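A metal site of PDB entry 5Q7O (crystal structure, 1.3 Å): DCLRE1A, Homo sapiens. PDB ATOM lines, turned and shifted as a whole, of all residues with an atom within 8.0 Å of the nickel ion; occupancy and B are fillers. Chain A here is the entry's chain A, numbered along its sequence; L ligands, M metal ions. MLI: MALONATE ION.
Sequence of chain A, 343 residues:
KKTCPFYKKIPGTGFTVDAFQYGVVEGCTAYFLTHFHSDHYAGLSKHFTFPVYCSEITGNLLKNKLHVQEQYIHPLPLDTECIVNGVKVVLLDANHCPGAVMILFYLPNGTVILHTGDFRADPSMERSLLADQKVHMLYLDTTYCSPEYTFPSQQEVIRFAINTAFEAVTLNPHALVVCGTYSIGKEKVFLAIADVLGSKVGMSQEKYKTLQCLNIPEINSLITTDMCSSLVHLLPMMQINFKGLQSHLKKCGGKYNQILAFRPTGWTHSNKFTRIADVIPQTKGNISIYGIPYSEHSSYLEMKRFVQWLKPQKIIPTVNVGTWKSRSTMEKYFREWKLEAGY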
ATOM      1  N   ASP A  18       8.885   8.620  -6.560  1.00  0.00           N
ATOM      2  CA  ASP A  18       8.723   9.169  -5.197  1.00  0.00           C
ATOM      3  C   ASP A  18       9.834   8.605  -4.226  1.00  0.00           C
ATOM      4  O   ASP A  18       9.519   8.188  -3.083  1.00  0.00           O
ATOM      5  CB  ASP A  18       7.325   8.977  -4.672  1.00  0.00           C
ATOM      6  CG  ASP A  18       6.234   9.640  -5.596  1.00  0.00           C
ATOM      7  OD1 ASP A  18       6.645  10.522  -6.407  1.00  0.00           O
ATOM      8  OD2 ASP A  18       5.031   9.323  -5.356  1.00  0.00           O
ATOM      9  N   THR A  34       5.348  12.154  -8.271  1.00  0.00           N
ATOM     10  CA  THR A  34       3.915  12.155  -8.622  1.00  0.00           C
ATOM     11  C   THR A  34       3.193  13.429  -8.169  1.00  0.00           C
ATOM     12  O   THR A  34       2.282  13.899  -8.868  1.00  0.00           O
ATOM     13  CB  THR A  34       3.173  10.936  -8.102  1.00  0.00           C
ATOM     14  OG1 THR A  34       3.215  10.910  -6.660  1.00  0.00           O
ATOM     15  CG2 THR A  34       3.689   9.587  -8.669  1.00  0.00           C
ATOM     16  N   HIS A  35       3.605  14.025  -7.021  1.00  0.00           N
ATOM     17  CA  HIS A  35       2.876  15.153  -6.439  1.00  0.00           C
ATOM     18  C   HIS A  35       3.670  15.769  -5.297  1.00  0.00           C
ATOM     19  O   HIS A  35       4.517  15.066  -4.674  1.00  0.00           O
ATOM     20  CB  HIS A  35       1.421  14.768  -6.034  1.00  0.00           C
ATOM     21  CG  HIS A  35       1.241  13.844  -4.884  1.00  0.00           C
ATOM     22  ND1 HIS A  35       1.572  12.521  -4.864  1.00  0.00           N
ATOM     23  CD2 HIS A  35       0.736  14.104  -3.644  1.00  0.00           C
ATOM     24  CE1 HIS A  35       1.288  12.008  -3.668  1.00  0.00           C
ATOM     25  NE2 HIS A  35       0.717  12.940  -2.957  1.00  0.00           N
ATOM     26  N   PHE A  36       3.320  16.982  -4.998  1.00  0.00           N
ATOM     27  CA  PHE A  36       4.071  17.763  -3.923  1.00  0.00           C
ATOM     28  C   PHE A  36       3.460  17.560  -2.515  1.00  0.00           C
ATOM     29  O   PHE A  36       2.854  18.527  -1.969  1.00  0.00           O
ATOM     30  CB  PHE A  36       4.127  19.253  -4.321  1.00  0.00           C
ATOM     31  CG  PHE A  36       5.137  20.099  -3.539  1.00  0.00           C
ATOM     32  CD1 PHE A  36       6.475  20.016  -3.857  1.00  0.00           C
ATOM     33  CD2 PHE A  36       4.730  20.982  -2.520  1.00  0.00           C
ATOM     34  CE1 PHE A  36       7.398  20.819  -3.151  1.00  0.00           C
ATOM     35  CE2 PHE A  36       5.657  21.752  -1.811  1.00  0.00           C
ATOM     36  CZ  PHE A  36       6.958  21.692  -2.136  1.00  0.00           C
ATOM     37  N   HIS A  37       3.534  16.363  -1.948  1.00  0.00           N
ATOM     38  CA  HIS A  37       3.223  16.072  -0.568  1.00  0.00           C
ATOM     39  C   HIS A  37       4.528  15.576   0.093  1.00  0.00           C
ATOM     40  O   HIS A  37       5.302  14.836  -0.547  1.00  0.00           O
ATOM     41  CB  HIS A  37       2.075  15.043  -0.379  1.00  0.00           C
ATOM     42  CG  HIS A  37       0.681  15.626  -0.528  1.00  0.00           C
ATOM     43  ND1 HIS A  37      -0.447  14.856  -0.695  1.00  0.00           N
ATOM     44  CD2 HIS A  37       0.265  16.917  -0.473  1.00  0.00           C
ATOM     45  CE1 HIS A  37      -1.514  15.649  -0.705  1.00  0.00           C
ATOM     46  NE2 HIS A  37      -1.103  16.893  -0.555  1.00  0.00           N
ATOM     47  N   SER A  38       4.727  15.930   1.387  1.00  0.00           N
ATOM     48  CA  SER A  38       6.072  15.759   2.014  1.00  0.00           C
ATOM     49  C   SER A  38       6.499  14.326   2.126  1.00  0.00           C
ATOM     50  O   SER A  38       7.714  14.096   1.941  1.00  0.00           O
ATOM     51  CB  SER A  38       6.189  16.516   3.350  1.00  0.00           C
ATOM     52  OG  SER A  38       5.179  16.054   4.188  1.00  0.00           O
ATOM     53  N   ASP A  39       5.596  13.368   2.327  1.00  0.00           N
ATOM     54  CA  ASP A  39       5.986  11.916   2.435  1.00  0.00           C
ATOM     55  C   ASP A  39       6.591  11.440   1.086  1.00  0.00           C
ATOM     56  O   ASP A  39       7.378  10.429   1.023  1.00  0.00           O
ATOM     57  CB  ASP A  39       4.862  10.975   2.887  1.00  0.00           C
ATOM     58  CG  ASP A  39       4.608  10.951   4.455  1.00  0.00           C
ATOM     59  OD1 ASP A  39       5.285  11.673   5.221  1.00  0.00           O
ATOM     60  OD2 ASP A  39       3.687  10.169   4.858  1.00  0.00           O
ATOM     61  N   HIS A  40       6.226  12.126  -0.013  1.00  0.00           N
ATOM     62  CA  HIS A  40       6.678  11.748  -1.369  1.00  0.00           C
ATOM     63  C   HIS A  40       7.869  12.495  -1.864  1.00  0.00           C
ATOM     64  O   HIS A  40       8.735  11.881  -2.512  1.00  0.00           O
ATOM     65  CB  HIS A  40       5.452  11.885  -2.355  1.00  0.00           C
ATOM     66  CG  HIS A  40       4.334  10.973  -2.011  1.00  0.00           C
ATOM     67  ND1 HIS A  40       4.054   9.798  -2.675  1.00  0.00           N
ATOM     68  CD2 HIS A  40       3.368  11.081  -1.063  1.00  0.00           C
ATOM     69  CE1 HIS A  40       3.058   9.171  -2.085  1.00  0.00           C
ATOM     70  NE2 HIS A  40       2.616   9.939  -1.107  1.00  0.00           N
ATOM     71  N   HIS A  96      -6.212  14.069  -7.193  1.00  0.00           N
ATOM     72  CA  HIS A  96      -5.719  14.167  -5.803  1.00  0.00           C
ATOM     73  C   HIS A  96      -5.557  15.619  -5.495  1.00  0.00           C
ATOM     74  O   HIS A  96      -6.624  16.264  -5.418  1.00  0.00           O
ATOM     75  CB  HIS A  96      -4.415  13.277  -5.693  1.00  0.00           C
ATOM     76  CG  HIS A  96      -3.789  13.166  -4.321  1.00  0.00           C
ATOM     77  ND1 HIS A  96      -4.516  12.772  -3.215  1.00  0.00           N
ATOM     78  CD2 HIS A  96      -2.544  13.458  -3.858  1.00  0.00           C
ATOM     79  CE1 HIS A  96      -3.721  12.727  -2.150  1.00  0.00           C
ATOM     80  NE2 HIS A  96      -2.513  13.149  -2.502  1.00  0.00           N
ATOM     81  N   CYS A  97      -4.375  16.168  -5.307  1.00  0.00           N
ATOM     82  CA  CYS A  97      -4.136  17.592  -5.058  1.00  0.00           C
ATOM     83  C   CYS A  97      -3.697  18.251  -6.324  1.00  0.00           C
ATOM     84  O   CYS A  97      -3.395  17.555  -7.313  1.00  0.00           O
ATOM     85  CB  CYS A  97      -3.109  17.719  -3.959  1.00  0.00           C
ATOM     86  SG  CYS A  97      -1.429  17.085  -4.372  1.00  0.00           S
ATOM     87  N   ALA A 100      -1.008  16.695  -9.129  1.00  0.00           N
ATOM     88  CA  ALA A 100      -0.815  15.273  -8.882  1.00  0.00           C
ATOM     89  C   ALA A 100      -1.119  14.457 -10.144  1.00  0.00           C
ATOM     90  O   ALA A 100      -2.147  14.693 -10.833  1.00  0.00           O
ATOM     91  CB  ALA A 100      -1.663  14.785  -7.717  1.00  0.00           C
ATOM     92  N   GLY A 117       0.349   6.888  -8.237  1.00  0.00           N
ATOM     93  CA  GLY A 117       0.671   7.846  -7.174  1.00  0.00           C
ATOM     94  C   GLY A 117      -0.393   7.787  -6.103  1.00  0.00           C
ATOM     95  O   GLY A 117      -0.920   6.745  -5.832  1.00  0.00           O
ATOM     96  N   ASP A 118      -0.720   8.950  -5.525  1.00  0.00           N
ATOM     97  CA  ASP A 118      -1.900   9.082  -4.698  1.00  0.00           C
ATOM     98  C   ASP A 118      -3.054   9.502  -5.639  1.00  0.00           C
ATOM     99  O   ASP A 118      -2.885  10.388  -6.495  1.00  0.00           O
ATOM    100  CB  ASP A 118      -1.725  10.136  -3.599  1.00  0.00           C
ATOM    101  CG  ASP A 118      -0.932   9.656  -2.380  1.00  0.00           C
ATOM    102  OD1 ASP A 118      -0.685   8.449  -2.251  1.00  0.00           O
ATOM    103  OD2 ASP A 118      -0.701  10.531  -1.534  1.00  0.00           O
ATOM    104  N   PHE A 119      -4.211   8.881  -5.504  1.00  0.00           N
ATOM    105  CA  PHE A 119      -5.355   9.213  -6.424  1.00  0.00           C
ATOM    106  C   PHE A 119      -6.691   9.051  -5.712  1.00  0.00           C
ATOM    107  O   PHE A 119      -6.875   8.277  -4.793  1.00  0.00           O
ATOM    108  CB  PHE A 119      -5.324   8.434  -7.780  1.00  0.00           C
ATOM    109  CG  PHE A 119      -5.906   7.007  -7.860  1.00  0.00           C
ATOM    110  CD1 PHE A 119      -6.597   6.577  -8.989  1.00  0.00           C
ATOM    111  CD2 PHE A 119      -5.688   6.034  -6.868  1.00  0.00           C
ATOM    112  CE1 PHE A 119      -7.036   5.258  -9.140  1.00  0.00           C
ATOM    113  CE2 PHE A 119      -6.172   4.710  -6.989  1.00  0.00           C
ATOM    114  CZ  PHE A 119      -6.861   4.343  -8.165  1.00  0.00           C
ATOM    115  N   ASP A 141      -2.496   3.030  -5.090  1.00  0.00           N
ATOM    116  CA  ASP A 141      -2.786   3.754  -3.807  1.00  0.00           C
ATOM    117  C   ASP A 141      -3.914   3.058  -3.083  1.00  0.00           C
ATOM    118  O   ASP A 141      -5.108   3.206  -3.449  1.00  0.00           O
ATOM    119  CB  ASP A 141      -3.140   5.224  -4.082  1.00  0.00           C
ATOM    120  CG  ASP A 141      -3.657   5.966  -2.901  1.00  0.00           C
ATOM    121  OD1 ASP A 141      -3.506   5.465  -1.759  1.00  0.00           O
ATOM    122  OD2 ASP A 141      -4.275   7.054  -3.116  1.00  0.00           O
ATOM    123  N   THR A 143      -4.676   3.380   0.264  1.00  0.00           N
ATOM    124  CA  THR A 143      -4.918   4.076   1.520  1.00  0.00           C
ATOM    125  C   THR A 143      -6.135   3.594   2.197  1.00  0.00           C
ATOM    126  O   THR A 143      -6.039   3.187   3.410  1.00  0.00           O
ATOM    127  CB  THR A 143      -4.952   5.632   1.296  1.00  0.00           C
ATOM    128  OG1 THR A 143      -3.691   6.098   0.856  1.00  0.00           O
ATOM    129  CG2 THR A 143      -5.239   6.354   2.601  1.00  0.00           C
ATOM    130  N   SER A 183      -0.981  21.290   4.044  1.00  0.00           N
ATOM    131  CA  SER A 183      -0.342  20.854   2.806  1.00  0.00           C
ATOM    132  C   SER A 183      -1.159  21.449   1.656  1.00  0.00           C
ATOM    133  O   SER A 183      -2.216  22.069   1.880  1.00  0.00           O
ATOM    134  CB  SER A 183      -0.370  19.332   2.674  1.00  0.00           C
ATOM    135  OG  SER A 183      -1.689  18.801   2.607  1.00  0.00           O
ATOM    136  N   ILE A 184      -0.748  21.246   0.420  1.00  0.00           N
ATOM    137  CA  ILE A 184      -1.632  21.535  -0.723  1.00  0.00           C
ATOM    138  C   ILE A 184      -2.705  20.447  -0.820  1.00  0.00           C
ATOM    139  O   ILE A 184      -2.579  19.358  -0.237  1.00  0.00           O
ATOM    140  CB  ILE A 184      -0.891  21.712  -2.051  1.00  0.00           C
ATOM    141  CG1 ILE A 184      -0.236  20.419  -2.514  1.00  0.00           C
ATOM    142  CG2 ILE A 184       0.137  22.859  -1.921  1.00  0.00           C
ATOM    143  CD1 ILE A 184       0.158  20.402  -3.964  1.00  0.00           C
ATOM    144  N   GLU A 296      -9.264  13.280  -0.583  1.00  0.00           N
ATOM    145  CA  GLU A 296      -8.565  13.205  -1.897  1.00  0.00           C
ATOM    146  C   GLU A 296      -7.964  11.805  -2.225  1.00  0.00           C
ATOM    147  O   GLU A 296      -7.091  11.667  -3.092  1.00  0.00           O
ATOM    148  CB  GLU A 296      -7.589  14.361  -2.098  1.00  0.00           C
ATOM    149  CG  GLU A 296      -8.316  15.754  -2.190  1.00  0.00           C
ATOM    150  CD  GLU A 296      -7.408  16.955  -2.483  1.00  0.00           C
ATOM    151  OE1 GLU A 296      -6.187  16.968  -2.194  1.00  0.00           O
ATOM    152  OE2 GLU A 296      -8.056  17.990  -2.986  1.00  0.00           O
ATOM    153  N   HIS A 297      -8.425  10.770  -1.492  1.00  0.00           N
ATOM    154  CA  HIS A 297      -8.131   9.354  -1.803  1.00  0.00           C
ATOM    155  C   HIS A 297      -9.398   8.581  -2.099  1.00  0.00           C
ATOM    156  O   HIS A 297     -10.501   8.909  -1.608  1.00  0.00           O
ATOM    157  CB  HIS A 297      -7.395   8.650  -0.638  1.00  0.00           C
ATOM    158  CG  HIS A 297      -6.052   9.193  -0.339  1.00  0.00           C
ATOM    159  ND1 HIS A 297      -4.878   8.786  -0.958  1.00  0.00           N
ATOM    160  CD2 HIS A 297      -5.642  10.087   0.613  1.00  0.00           C
ATOM    161  CE1 HIS A 297      -3.832   9.427  -0.459  1.00  0.00           C
ATOM    162  NE2 HIS A 297      -4.272  10.183   0.526  1.00  0.00           N
HETATM  163  C1  MLI L   1      -0.658  12.560   2.205  1.00  0.00           C
HETATM  164  C2  MLI L   1      -1.991  12.227   1.595  1.00  0.00           C
HETATM  165  C3  MLI L   1       0.558  12.011   1.487  1.00  0.00           C
HETATM  166  O6  MLI L   1      -2.941  11.892   2.312  1.00  0.00           O
HETATM  167  O7  MLI L   1      -2.096  12.434   0.363  1.00  0.00           O
HETATM  168  O8  MLI L   1       0.691  12.185   0.222  1.00  0.00           O
HETATM  169  O9  MLI L   1       1.484  11.546   2.237  1.00  0.00           O
HETATM  170 NI    NI M   1      -0.680  12.695  -1.203  1.00  0.00          NI
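Four residues have an atom within 4 Å of the nickel ion: His 35, His 37, His 96 and Asp 118. The nearest printed residue that does not touch the nickel ion is His 40 (4.3 Å).
The nickel ion is bound by an oxygen (O8) of the ligand, an oxygen (O7) of the ligand, the side-chain carboxylate of Asp 118, a ring nitrogen (ND1) of His 37, a ring nitrogen (NE2) of His 35 and a ring nitrogen (NE2) of His 96.
A ring nitrogen (NE2) of His 40 lies close to the side-chain carboxylate (OD2) of Asp 118, 3.4 Å away. A ring nitrogen (NE2) of His 37 is in hydrogen-bond range of the backbone carbonyl oxygen (O) of Ile 184, 2.9 Å away. A ring nitrogen (ND1) of His 35 lies within hydrogen-bond range of the side-chain hydroxyl of Thr 34, 2.9 Å away. A ring nitrogen (ND1) of His 96 sits at hydrogen-bond distance from the backbone carbonyl oxygen of Glu 296, 2.8 Å away.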
